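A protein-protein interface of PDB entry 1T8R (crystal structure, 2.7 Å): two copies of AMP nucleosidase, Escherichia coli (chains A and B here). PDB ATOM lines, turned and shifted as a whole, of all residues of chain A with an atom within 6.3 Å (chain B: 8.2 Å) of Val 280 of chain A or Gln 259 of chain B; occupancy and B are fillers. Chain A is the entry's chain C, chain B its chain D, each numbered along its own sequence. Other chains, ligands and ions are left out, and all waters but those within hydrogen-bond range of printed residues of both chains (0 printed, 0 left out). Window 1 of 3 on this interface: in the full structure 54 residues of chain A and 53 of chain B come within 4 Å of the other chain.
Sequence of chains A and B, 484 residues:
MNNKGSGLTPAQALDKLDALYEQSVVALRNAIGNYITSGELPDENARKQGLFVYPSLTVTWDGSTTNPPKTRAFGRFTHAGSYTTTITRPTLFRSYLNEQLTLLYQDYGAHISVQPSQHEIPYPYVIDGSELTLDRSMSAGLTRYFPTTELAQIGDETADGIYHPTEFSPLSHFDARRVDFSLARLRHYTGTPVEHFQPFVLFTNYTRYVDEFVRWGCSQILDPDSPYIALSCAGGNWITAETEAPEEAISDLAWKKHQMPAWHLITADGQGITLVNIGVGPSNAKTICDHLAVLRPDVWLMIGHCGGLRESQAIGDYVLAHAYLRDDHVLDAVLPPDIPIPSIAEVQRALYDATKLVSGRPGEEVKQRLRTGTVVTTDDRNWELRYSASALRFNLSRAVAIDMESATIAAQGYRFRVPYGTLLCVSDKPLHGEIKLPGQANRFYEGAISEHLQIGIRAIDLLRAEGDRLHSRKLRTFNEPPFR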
ATOM      1  N   ASN A 205      19.898  25.379   3.802  1.00  0.00           N
ATOM      2  CA  ASN A 205      20.991  24.773   4.556  1.00  0.00           C
ATOM      3  C   ASN A 205      22.335  25.031   3.889  1.00  0.00           C
ATOM      4  O   ASN A 205      23.301  24.307   4.125  1.00  0.00           O
ATOM      5  CB  ASN A 205      20.775  23.259   4.685  1.00  0.00           C
ATOM      6  CG  ASN A 205      20.583  22.586   3.355  1.00  0.00           C
ATOM      7  OD1 ASN A 205      20.802  23.183   2.294  1.00  0.00           O
ATOM      8  ND2 ASN A 205      20.179  21.332   3.392  1.00  0.00           N
ATOM      9  N   ILE A 278      18.968  27.823   8.305  1.00  0.00           N
ATOM     10  CA  ILE A 278      18.942  26.983   9.487  1.00  0.00           C
ATOM     11  C   ILE A 278      20.213  26.184   9.701  1.00  0.00           C
ATOM     12  O   ILE A 278      20.415  25.589  10.755  1.00  0.00           O
ATOM     13  CB  ILE A 278      17.731  26.053   9.433  1.00  0.00           C
ATOM     14  CG1 ILE A 278      17.837  25.102   8.246  1.00  0.00           C
ATOM     15  CG2 ILE A 278      16.481  26.890   9.288  1.00  0.00           C
ATOM     16  CD1 ILE A 278      16.653  24.188   8.136  1.00  0.00           C
ATOM     17  N   GLY A 279      21.086  26.186   8.711  1.00  0.00           N
ATOM     18  CA  GLY A 279      22.314  25.447   8.872  1.00  0.00           C
ATOM     19  C   GLY A 279      22.072  23.987   8.596  1.00  0.00           C
ATOM     20  O   GLY A 279      21.246  23.650   7.746  1.00  0.00           O
ATOM     21  N   VAL A 280      22.755  23.119   9.334  1.00  0.00           N
ATOM     22  CA  VAL A 280      22.630  21.688   9.112  1.00  0.00           C
ATOM     23  C   VAL A 280      22.322  20.893  10.375  1.00  0.00           C
ATOM     24  O   VAL A 280      22.868  21.167  11.442  1.00  0.00           O
ATOM     25  CB  VAL A 280      23.931  21.146   8.473  1.00  0.00           C
ATOM     26  CG1 VAL A 280      25.110  21.424   9.396  1.00  0.00           C
ATOM     27  CG2 VAL A 280      23.810  19.664   8.205  1.00  0.00           C
ATOM     28  N   GLY A 281      21.441  19.901  10.239  1.00  0.00           N
ATOM     29  CA  GLY A 281      21.088  19.062  11.371  1.00  0.00           C
ATOM     30  C   GLY A 281      19.640  19.166  11.797  1.00  0.00           C
ATOM     31  O   GLY A 281      19.021  20.215  11.642  1.00  0.00           O
ATOM     32  N   PRO A 282      19.064  18.082  12.328  1.00  0.00           N
ATOM     33  CA  PRO A 282      17.669  18.069  12.778  1.00  0.00           C
ATOM     34  C   PRO A 282      17.437  18.965  13.996  1.00  0.00           C
ATOM     35  O   PRO A 282      16.370  19.552  14.157  1.00  0.00           O
ATOM     36  CB  PRO A 282      17.428  16.593  13.104  1.00  0.00           C
ATOM     37  CG  PRO A 282      18.348  15.874  12.187  1.00  0.00           C
ATOM     38  CD  PRO A 282      19.609  16.715  12.281  1.00  0.00           C
ATOM     39  N   SER A 283      18.434  19.050  14.865  1.00  0.00           N
ATOM     40  CA  SER A 283      18.337  19.871  16.068  1.00  0.00           C
ATOM     41  C   SER A 283      17.986  21.306  15.761  1.00  0.00           C
ATOM     42  O   SER A 283      17.127  21.887  16.411  1.00  0.00           O
ATOM     43  CB  SER A 283      19.651  19.858  16.846  1.00  0.00           C
ATOM     44  OG  SER A 283      19.802  18.640  17.543  1.00  0.00           O
ATOM     45  N   ASN A 284      18.665  21.884  14.783  1.00  0.00           N
ATOM     46  CA  ASN A 284      18.404  23.258  14.428  1.00  0.00           C
ATOM     47  C   ASN A 284      17.047  23.427  13.777  1.00  0.00           C
ATOM     48  O   ASN A 284      16.313  24.374  14.068  1.00  0.00           O
ATOM     49  CB  ASN A 284      19.489  23.762  13.489  1.00  0.00           C
ATOM     50  CG  ASN A 284      20.700  24.293  14.227  1.00  0.00           C
ATOM     51  OD1 ASN A 284      21.564  24.923  13.622  1.00  0.00           O
ATOM     52  ND2 ASN A 284      20.768  24.045  15.532  1.00  0.00           N
ATOM     53  N   HIS A 305      20.135  21.452  -0.377  1.00  0.00           N
ATOM     54  CA  HIS A 305      20.771  20.376  -1.103  1.00  0.00           C
ATOM     55  C   HIS A 305      20.505  19.029  -0.422  1.00  0.00           C
ATOM     56  O   HIS A 305      20.067  18.972   0.743  1.00  0.00           O
ATOM     57  CB  HIS A 305      22.264  20.646  -1.170  1.00  0.00           C
ATOM     58  CG  HIS A 305      22.902  20.734   0.174  1.00  0.00           C
ATOM     59  ND1 HIS A 305      23.093  19.631   0.978  1.00  0.00           N
ATOM     60  CD2 HIS A 305      23.337  21.798   0.886  1.00  0.00           C
ATOM     61  CE1 HIS A 305      23.616  20.012   2.130  1.00  0.00           C
ATOM     62  NE2 HIS A 305      23.773  21.324   2.099  1.00  0.00           N
ATOM     63  N   ARG A 381      25.413  12.649   9.867  1.00  0.00           N
ATOM     64  CA  ARG A 381      26.032  13.114   8.639  1.00  0.00           C
ATOM     65  C   ARG A 381      26.925  12.075   7.966  1.00  0.00           C
ATOM     66  O   ARG A 381      26.991  12.023   6.742  1.00  0.00           O
ATOM     67  CB  ARG A 381      26.841  14.381   8.867  1.00  0.00           C
ATOM     68  CG  ARG A 381      27.701  14.708   7.650  1.00  0.00           C
ATOM     69  CD  ARG A 381      27.443  16.102   7.114  1.00  0.00           C
ATOM     70  NE  ARG A 381      27.746  17.114   8.117  1.00  0.00           N
ATOM     71  CZ  ARG A 381      27.666  18.422   7.903  1.00  0.00           C
ATOM     72  NH1 ARG A 381      27.290  18.877   6.705  1.00  0.00           N
ATOM     73  NH2 ARG A 381      27.965  19.270   8.884  1.00  0.00           N
ATOM     74  N   MET A 404      19.283  16.285   5.877  1.00  0.00           N
ATOM     75  CA  MET A 404      19.244  16.369   7.321  1.00  0.00           C
ATOM     76  C   MET A 404      18.270  17.338   7.967  1.00  0.00           C
ATOM     77  O   MET A 404      18.318  17.528   9.179  1.00  0.00           O
ATOM     78  CB  MET A 404      20.648  16.635   7.834  1.00  0.00           C
ATOM     79  CG  MET A 404      21.592  15.504   7.516  1.00  0.00           C
ATOM     80  SD  MET A 404      23.359  15.802   8.211  1.00  0.00           S
ATOM     81  CE  MET A 404      23.027  15.501  10.100  1.00  0.00           C
ATOM     82  N   GLU A 405      17.367  17.929   7.195  1.00  0.00           N
ATOM     83  CA  GLU A 405      16.414  18.868   7.774  1.00  0.00           C
ATOM     84  C   GLU A 405      14.956  18.623   7.379  1.00  0.00           C
ATOM     85  O   GLU A 405      14.048  18.837   8.188  1.00  0.00           O
ATOM     86  CB  GLU A 405      16.788  20.295   7.390  1.00  0.00           C
ATOM     87  CG  GLU A 405      18.152  20.771   7.851  1.00  0.00           C
ATOM     88  CD  GLU A 405      19.313  20.277   6.981  1.00  0.00           C
ATOM     89  OE1 GLU A 405      19.114  20.054   5.757  1.00  0.00           O
ATOM     90  OE2 GLU A 405      20.439  20.138   7.523  1.00  0.00           O
ATOM     91  N   PRO A 438      28.563  20.064   0.229  1.00  0.00           N
ATOM     92  CA  PRO A 438      28.227  21.461  -0.063  1.00  0.00           C
ATOM     93  C   PRO A 438      29.201  22.451   0.571  1.00  0.00           C
ATOM     94  O   PRO A 438      29.364  22.493   1.794  1.00  0.00           O
ATOM     95  CB  PRO A 438      26.809  21.583   0.474  1.00  0.00           C
ATOM     96  CG  PRO A 438      26.241  20.251   0.110  1.00  0.00           C
ATOM     97  CD  PRO A 438      27.342  19.298   0.543  1.00  0.00           C
ATOM     98  N   ARG B 187      39.745  18.953   6.695  1.00  0.00           N
ATOM     99  CA  ARG B 187      40.154  20.180   6.041  1.00  0.00           C
ATOM    100  C   ARG B 187      38.943  21.051   5.704  1.00  0.00           C
ATOM    101  O   ARG B 187      38.928  22.227   6.026  1.00  0.00           O
ATOM    102  CB  ARG B 187      40.944  19.861   4.773  1.00  0.00           C
ATOM    103  CG  ARG B 187      41.296  21.088   3.975  1.00  0.00           C
ATOM    104  CD  ARG B 187      42.536  20.882   3.128  1.00  0.00           C
ATOM    105  NE  ARG B 187      42.945  22.122   2.463  1.00  0.00           N
ATOM    106  CZ  ARG B 187      43.162  23.284   3.085  1.00  0.00           C
ATOM    107  NH1 ARG B 187      43.010  23.390   4.404  1.00  0.00           N
ATOM    108  NH2 ARG B 187      43.533  24.352   2.386  1.00  0.00           N
ATOM    109  N   HIS B 188      37.928  20.474   5.071  1.00  0.00           N
ATOM    110  CA  HIS B 188      36.732  21.218   4.696  1.00  0.00           C
ATOM    111  C   HIS B 188      35.997  21.847   5.883  1.00  0.00           C
ATOM    112  O   HIS B 188      35.684  23.036   5.857  1.00  0.00           O
ATOM    113  CB  HIS B 188      35.771  20.302   3.929  1.00  0.00           C
ATOM    114  CG  HIS B 188      34.444  20.931   3.603  1.00  0.00           C
ATOM    115  ND1 HIS B 188      34.311  22.011   2.753  1.00  0.00           N
ATOM    116  CD2 HIS B 188      33.183  20.601   3.987  1.00  0.00           C
ATOM    117  CE1 HIS B 188      33.031  22.317   2.625  1.00  0.00           C
ATOM    118  NE2 HIS B 188      32.325  21.476   3.361  1.00  0.00           N
ATOM    119  N   TYR B 189      35.718  21.054   6.916  1.00  0.00           N
ATOM    120  CA  TYR B 189      34.995  21.538   8.094  1.00  0.00           C
ATOM    121  C   TYR B 189      35.797  22.509   8.944  1.00  0.00           C
ATOM    122  O   TYR B 189      35.271  23.443   9.540  1.00  0.00           O
ATOM    123  CB  TYR B 189      34.606  20.372   9.014  1.00  0.00           C
ATOM    124  CG  TYR B 189      33.553  19.433   8.491  1.00  0.00           C
ATOM    125  CD1 TYR B 189      32.332  19.915   8.038  1.00  0.00           C
ATOM    126  CD2 TYR B 189      33.756  18.057   8.500  1.00  0.00           C
ATOM    127  CE1 TYR B 189      31.338  19.058   7.613  1.00  0.00           C
ATOM    128  CE2 TYR B 189      32.765  17.189   8.076  1.00  0.00           C
ATOM    129  CZ  TYR B 189      31.554  17.702   7.634  1.00  0.00           C
ATOM    130  OH  TYR B 189      30.549  16.861   7.223  1.00  0.00           O
ATOM    131  N   THR B 190      37.087  22.262   9.001  1.00  0.00           N
ATOM    132  CA  THR B 190      37.981  23.023   9.828  1.00  0.00           C
ATOM    133  C   THR B 190      38.625  24.270   9.226  1.00  0.00           C
ATOM    134  O   THR B 190      38.979  25.190   9.968  1.00  0.00           O
ATOM    135  CB  THR B 190      39.038  22.036  10.349  1.00  0.00           C
ATOM    136  OG1 THR B 190      38.560  21.450  11.567  1.00  0.00           O
ATOM    137  CG2 THR B 190      40.367  22.682  10.541  1.00  0.00           C
ATOM    138  N   GLY B 191      38.749  24.309   7.896  1.00  0.00           N
ATOM    139  CA  GLY B 191      39.390  25.436   7.237  1.00  0.00           C
ATOM    140  C   GLY B 191      40.859  25.468   7.642  1.00  0.00           C
ATOM    141  O   GLY B 191      41.478  26.528   7.787  1.00  0.00           O
ATOM    142  N   LEU B 253      35.095  35.829   8.319  1.00  0.00           N
ATOM    143  CA  LEU B 253      34.678  35.021   7.178  1.00  0.00           C
ATOM    144  C   LEU B 253      34.778  33.518   7.473  1.00  0.00           C
ATOM    145  O   LEU B 253      34.084  32.711   6.853  1.00  0.00           O
ATOM    146  CB  LEU B 253      35.534  35.378   5.955  1.00  0.00           C
ATOM    147  CG  LEU B 253      35.330  34.598   4.649  1.00  0.00           C
ATOM    148  CD1 LEU B 253      33.894  34.731   4.176  1.00  0.00           C
ATOM    149  CD2 LEU B 253      36.295  35.126   3.588  1.00  0.00           C
ATOM    150  N   ALA B 254      35.632  33.152   8.426  1.00  0.00           N
ATOM    151  CA  ALA B 254      35.829  31.757   8.788  1.00  0.00           C
ATOM    152  C   ALA B 254      34.530  31.073   9.192  1.00  0.00           C
ATOM    153  O   ALA B 254      34.253  29.952   8.762  1.00  0.00           O
ATOM    154  CB  ALA B 254      36.853  31.648   9.914  1.00  0.00           C
ATOM    155  N   TRP B 255      33.732  31.754  10.010  1.00  0.00           N
ATOM    156  CA  TRP B 255      32.467  31.192  10.476  1.00  0.00           C
ATOM    157  C   TRP B 255      31.400  31.040   9.411  1.00  0.00           C
ATOM    158  O   TRP B 255      30.379  30.392   9.639  1.00  0.00           O
ATOM    159  CB  TRP B 255      31.922  32.002  11.644  1.00  0.00           C
ATOM    160  CG  TRP B 255      32.486  31.536  12.933  1.00  0.00           C
ATOM    161  CD1 TRP B 255      32.155  30.392  13.616  1.00  0.00           C
ATOM    162  CD2 TRP B 255      33.541  32.152  13.666  1.00  0.00           C
ATOM    163  NE1 TRP B 255      32.948  30.262  14.731  1.00  0.00           N
ATOM    164  CE2 TRP B 255      33.808  31.328  14.787  1.00  0.00           C
ATOM    165  CE3 TRP B 255      34.289  33.318  13.485  1.00  0.00           C
ATOM    166  CZ2 TRP B 255      34.792  31.638  15.721  1.00  0.00           C
ATOM    167  CZ3 TRP B 255      35.262  33.626  14.407  1.00  0.00           C
ATOM    168  CH2 TRP B 255      35.509  32.789  15.517  1.00  0.00           C
ATOM    169  N   LYS B 256      31.629  31.627   8.243  1.00  0.00           N
ATOM    170  CA  LYS B 256      30.669  31.495   7.159  1.00  0.00           C
ATOM    171  C   LYS B 256      31.140  30.363   6.264  1.00  0.00           C
ATOM    172  O   LYS B 256      30.341  29.577   5.759  1.00  0.00           O
ATOM    173  CB  LYS B 256      30.576  32.789   6.342  1.00  0.00           C
ATOM    174  CG  LYS B 256      29.624  32.700   5.143  1.00  0.00           C
ATOM    175  CD  LYS B 256      29.655  33.960   4.272  1.00  0.00           C
ATOM    176  CE  LYS B 256      28.729  33.827   3.061  1.00  0.00           C
ATOM    177  NZ  LYS B 256      28.655  35.069   2.236  1.00  0.00           N
ATOM    178  N   LYS B 257      32.454  30.275   6.085  1.00  0.00           N
ATOM    179  CA  LYS B 257      33.035  29.254   5.222  1.00  0.00           C
ATOM    180  C   LYS B 257      33.142  27.880   5.846  1.00  0.00           C
ATOM    181  O   LYS B 257      32.994  26.875   5.157  1.00  0.00           O
ATOM    182  CB  LYS B 257      34.430  29.675   4.765  1.00  0.00           C
ATOM    183  CG  LYS B 257      34.478  30.762   3.708  1.00  0.00           C
ATOM    184  CD  LYS B 257      35.938  31.057   3.337  1.00  0.00           C
ATOM    185  CE  LYS B 257      36.054  32.111   2.242  1.00  0.00           C
ATOM    186  NZ  LYS B 257      37.474  32.466   1.932  1.00  0.00           N
ATOM    187  N   HIS B 258      33.404  27.833   7.148  1.00  0.00           N
ATOM    188  CA  HIS B 258      33.578  26.552   7.816  1.00  0.00           C
ATOM    189  C   HIS B 258      32.645  26.296   8.980  1.00  0.00           C
ATOM    190  O   HIS B 258      32.470  27.143   9.852  1.00  0.00           O
ATOM    191  CB  HIS B 258      35.028  26.411   8.265  1.00  0.00           C
ATOM    192  CG  HIS B 258      36.011  26.799   7.210  1.00  0.00           C
ATOM    193  ND1 HIS B 258      36.589  28.050   7.156  1.00  0.00           N
ATOM    194  CD2 HIS B 258      36.471  26.125   6.129  1.00  0.00           C
ATOM    195  CE1 HIS B 258      37.363  28.130   6.089  1.00  0.00           C
ATOM    196  NE2 HIS B 258      37.309  26.976   5.448  1.00  0.00           N
ATOM    197  N   GLN B 259      32.070  25.099   8.985  1.00  0.00           N
ATOM    198  CA  GLN B 259      31.136  24.687  10.010  1.00  0.00           C
ATOM    199  C   GLN B 259      31.756  24.468  11.378  1.00  0.00           C
ATOM    200  O   GLN B 259      31.118  24.708  12.396  1.00  0.00           O
ATOM    201  CB  GLN B 259      30.423  23.428   9.557  1.00  0.00           C
ATOM    202  CG  GLN B 259      29.527  23.647   8.366  1.00  0.00           C
ATOM    203  CD  GLN B 259      28.748  22.403   8.031  1.00  0.00           C
ATOM    204  OE1 GLN B 259      28.228  21.735   8.930  1.00  0.00           O
ATOM    205  NE2 GLN B 259      28.654  22.078   6.746  1.00  0.00           N
ATOM    206  N   MET B 260      33.000  24.013  11.409  1.00  0.00           N
ATOM    207  CA  MET B 260      33.673  23.769  12.668  1.00  0.00           C
ATOM    208  C   MET B 260      35.107  24.246  12.603  1.00  0.00           C
ATOM    209  O   MET B 260      36.040  23.456  12.557  1.00  0.00           O
ATOM    210  CB  MET B 260      33.591  22.289  13.003  1.00  0.00           C
ATOM    211  CG  MET B 260      32.163  21.870  13.301  1.00  0.00           C
ATOM    212  SD  MET B 260      31.803  19.985  13.158  1.00  0.00           S
ATOM    213  CE  MET B 260      31.386  19.925  11.268  1.00  0.00           C
ATOM    214  N   PRO B 261      35.290  25.572  12.619  1.00  0.00           N
ATOM    215  CA  PRO B 261      36.567  26.289  12.559  1.00  0.00           C
ATOM    216  C   PRO B 261      37.544  25.737  13.580  1.00  0.00           C
ATOM    217  O   PRO B 261      37.152  25.406  14.689  1.00  0.00           O
ATOM    218  CB  PRO B 261      36.175  27.728  12.904  1.00  0.00           C
ATOM    219  CG  PRO B 261      34.753  27.814  12.520  1.00  0.00           C
ATOM    220  CD  PRO B 261      34.204  26.496  12.984  1.00  0.00           C
ATOM    221  N   ALA B 262      38.812  25.641  13.208  1.00  0.00           N
ATOM    222  CA  ALA B 262      39.830  25.148  14.125  1.00  0.00           C
ATOM    223  C   ALA B 262      41.018  26.109  14.206  1.00  0.00           C
ATOM    224  O   ALA B 262      41.257  26.919  13.312  1.00  0.00           O
ATOM    225  CB  ALA B 262      40.307  23.763  13.702  1.00  0.00           C
ATOM    226  N   VAL B 276      38.866  23.244  18.399  1.00  0.00           N
ATOM    227  CA  VAL B 276      37.854  23.192  17.365  1.00  0.00           C
ATOM    228  C   VAL B 276      36.549  23.697  17.951  1.00  0.00           C
ATOM    229  O   VAL B 276      36.145  23.275  19.031  1.00  0.00           O
ATOM    230  CB  VAL B 276      37.646  21.760  16.851  1.00  0.00           C
ATOM    231  CG1 VAL B 276      36.743  21.773  15.641  1.00  0.00           C
ATOM    232  CG2 VAL B 276      38.970  21.138  16.504  1.00  0.00           C
ATOM    233  N   ASN B 277      35.909  24.629  17.261  1.00  0.00           N
ATOM    234  CA  ASN B 277      34.633  25.146  17.724  1.00  0.00           C
ATOM    235  C   ASN B 277      33.623  24.298  16.977  1.00  0.00           C
ATOM    236  O   ASN B 277      33.318  24.551  15.817  1.00  0.00           O
ATOM    237  CB  ASN B 277      34.478  26.622  17.361  1.00  0.00           C
ATOM    238  CG  ASN B 277      33.227  27.246  17.961  1.00  0.00           C
ATOM    239  OD1 ASN B 277      33.000  27.177  19.172  1.00  0.00           O
ATOM    240  ND2 ASN B 277      32.417  27.870  17.118  1.00  0.00           N
ATOM    241  N   ILE B 278      33.123  23.272  17.652  1.00  0.00           N
ATOM    242  CA  ILE B 278      32.191  22.347  17.044  1.00  0.00           C
ATOM    243  C   ILE B 278      30.792  22.906  16.901  1.00  0.00           C
ATOM    244  O   ILE B 278      29.949  22.350  16.195  1.00  0.00           O
ATOM    245  CB  ILE B 278      32.175  21.021  17.828  1.00  0.00           C
ATOM    246  CG1 ILE B 278      31.678  21.225  19.253  1.00  0.00           C
ATOM    247  CG2 ILE B 278      33.580  20.463  17.878  1.00  0.00           C
ATOM    248  CD1 ILE B 278      31.766  19.980  20.083  1.00  0.00           C
ATOM    249  N   GLY B 279      30.540  24.028  17.549  1.00  0.00           N
ATOM    250  CA  GLY B 279      29.222  24.595  17.445  1.00  0.00           C
ATOM    251  C   GLY B 279      28.318  23.904  18.435  1.00  0.00           C
ATOM    252  O   GLY B 279      28.763  23.509  19.518  1.00  0.00           O
ATOM    253  N   VAL B 280      27.060  23.715  18.050  1.00  0.00           N
ATOM    254  CA  VAL B 280      26.080  23.117  18.947  1.00  0.00           C
ATOM    255  C   VAL B 280      25.334  21.940  18.333  1.00  0.00           C
ATOM    256  O   VAL B 280      25.031  21.933  17.132  1.00  0.00           O
ATOM    257  CB  VAL B 280      25.053  24.206  19.404  1.00  0.00           C
ATOM    258  CG1 VAL B 280      24.398  24.820  18.187  1.00  0.00           C
ATOM    259  CG2 VAL B 280      24.000  23.610  20.330  1.00  0.00           C
ATOM    260  N   GLY B 281      25.045  20.943  19.168  1.00  0.00           N
ATOM    261  CA  GLY B 281      24.317  19.780  18.702  1.00  0.00           C
ATOM    262  C   GLY B 281      25.132  18.506  18.664  1.00  0.00           C
ATOM    263  O   GLY B 281      26.347  18.539  18.465  1.00  0.00           O
ATOM    264  N   SER B 283      24.919  16.078  16.430  1.00  0.00           N
ATOM    265  CA  SER B 283      25.300  15.774  15.052  1.00  0.00           C
ATOM    266  C   SER B 283      26.712  16.232  14.729  1.00  0.00           C
ATOM    267  O   SER B 283      27.506  15.476  14.185  1.00  0.00           O
ATOM    268  CB  SER B 283      24.337  16.433  14.058  1.00  0.00           C
ATOM    269  OG  SER B 283      23.128  15.706  13.930  1.00  0.00           O
ATOM    270  N   ASN B 284      27.024  17.476  15.054  1.00  0.00           N
ATOM    271  CA  ASN B 284      28.347  17.983  14.776  1.00  0.00           C
ATOM    272  C   ASN B 284      29.403  17.287  15.609  1.00  0.00           C
ATOM    273  O   ASN B 284      30.464  16.921  15.111  1.00  0.00           O
ATOM    274  CB  ASN B 284      28.396  19.485  15.039  1.00  0.00           C
ATOM    275  CG  ASN B 284      27.907  20.294  13.862  1.00  0.00           C
ATOM    276  OD1 ASN B 284      28.065  21.508  13.834  1.00  0.00           O
ATOM    277  ND2 ASN B 284      27.311  19.625  12.881  1.00  0.00           N
ATOM    278  N   THR B 287      30.156  14.005  14.107  1.00  0.00           N
ATOM    279  CA  THR B 287      30.859  14.178  12.849  1.00  0.00           C
ATOM    280  C   THR B 287      32.321  14.543  13.005  1.00  0.00           C
ATOM    281  O   THR B 287      33.190  13.904  12.426  1.00  0.00           O
ATOM    282  CB  THR B 287      30.190  15.263  11.986  1.00  0.00           C
ATOM    283  OG1 THR B 287      28.835  14.891  11.744  1.00  0.00           O
ATOM    284  CG2 THR B 287      30.909  15.425  10.645  1.00  0.00           C
ATOM    285  N   ILE B 288      32.603  15.566  13.792  1.00  0.00           N
ATOM    286  CA  ILE B 288      33.974  15.980  13.930  1.00  0.00           C
ATOM    287  C   ILE B 288      34.833  14.857  14.494  1.00  0.00           C
ATOM    288  O   ILE B 288      35.918  14.589  13.976  1.00  0.00           O
ATOM    289  CB  ILE B 288      34.082  17.285  14.773  1.00  0.00           C
ATOM    290  CG1 ILE B 288      35.477  17.868  14.611  1.00  0.00           C
ATOM    291  CG2 ILE B 288      33.762  17.037  16.222  1.00  0.00           C
ATOM    292  CD1 ILE B 288      35.792  18.160  13.175  1.00  0.00           C
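Positions printed for both chains: 278, 279, 280, 281, 283 and 284.
Of chain B, only Gln 259 comes within 4 Å of Val 280 of chain A.
Of the printed residues of chain A, Gln 259 of chain B touches Val 280 (3.2 Å) and Arg 381 (2.5 Å).
No residue of chain B comes within 4 Å of Gly 279 of chain A.
No residue of chain B comes within 4 Å of Gly 281 of chain A.
Of the printed residues of chain A, Ser 283 of chain B touches Met 404.
Of the printed residues of chain B, Arg 381 of chain A touches Tyr 189, Gln 259 and Thr 287.
Printed residues of chain B within 4 Å of Met 404 of chain A: Ser 283 (3.8 Å).
Gly 281 of chain B touches none of the printed residues of chain A.
Lys 257 of chain B touches none of the printed residues of chain A.
The nearest printed residue of chain A that does not touch Ser 283 of chain B is Pro 282 of chain A (4.02 Å).
The side-chain hydroxyl of Tyr 189 of chain B is in hydrogen-bond range of the guanidinium group of Arg 381 of chain A (3.0 Å).
NH2 of Arg 381 of chain A lies within hydrogen-bond range of OE1 of Gln 259 of chain B, 2.5 Å away.
The side-chain hydroxyl (OG1) of Thr 287 of chain B sits at hydrogen-bond distance from the backbone carbonyl oxygen (O) of Ser 283 of chain B (2.8 Å).
The backbone carbonyl oxygen (O) of Tyr 189 of chain B sits at hydrogen-bond distance from the backbone NH (N) of Met 260 of chain B (3.0 Å).
Hydrophobic or aromatic side chains of chain B that line the printed part of chain A: His 188 and Tyr 189.
Hydrophobic or aromatic side chains of chain A within 4 Å of the printed part of chain B: Val 280 and Met 404.
Along chain A the printed residues that touch a printed residue of chain B span positions 280 to 438.
Among the printed residues, 6 pairs touch across the chains.
Gln 259 of chain B touches Val 280 of chain A (OE1 to CG1, 3.2 Å).
CB of Arg 381 of chain A touches OG1 of Thr 287 of chain B (3.5 Å).
Met 404 of chain A touches Ser 283 of chain B (CE to OG, 3.8 Å).
Pro 438 of chain A touches His 188 of chain B.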
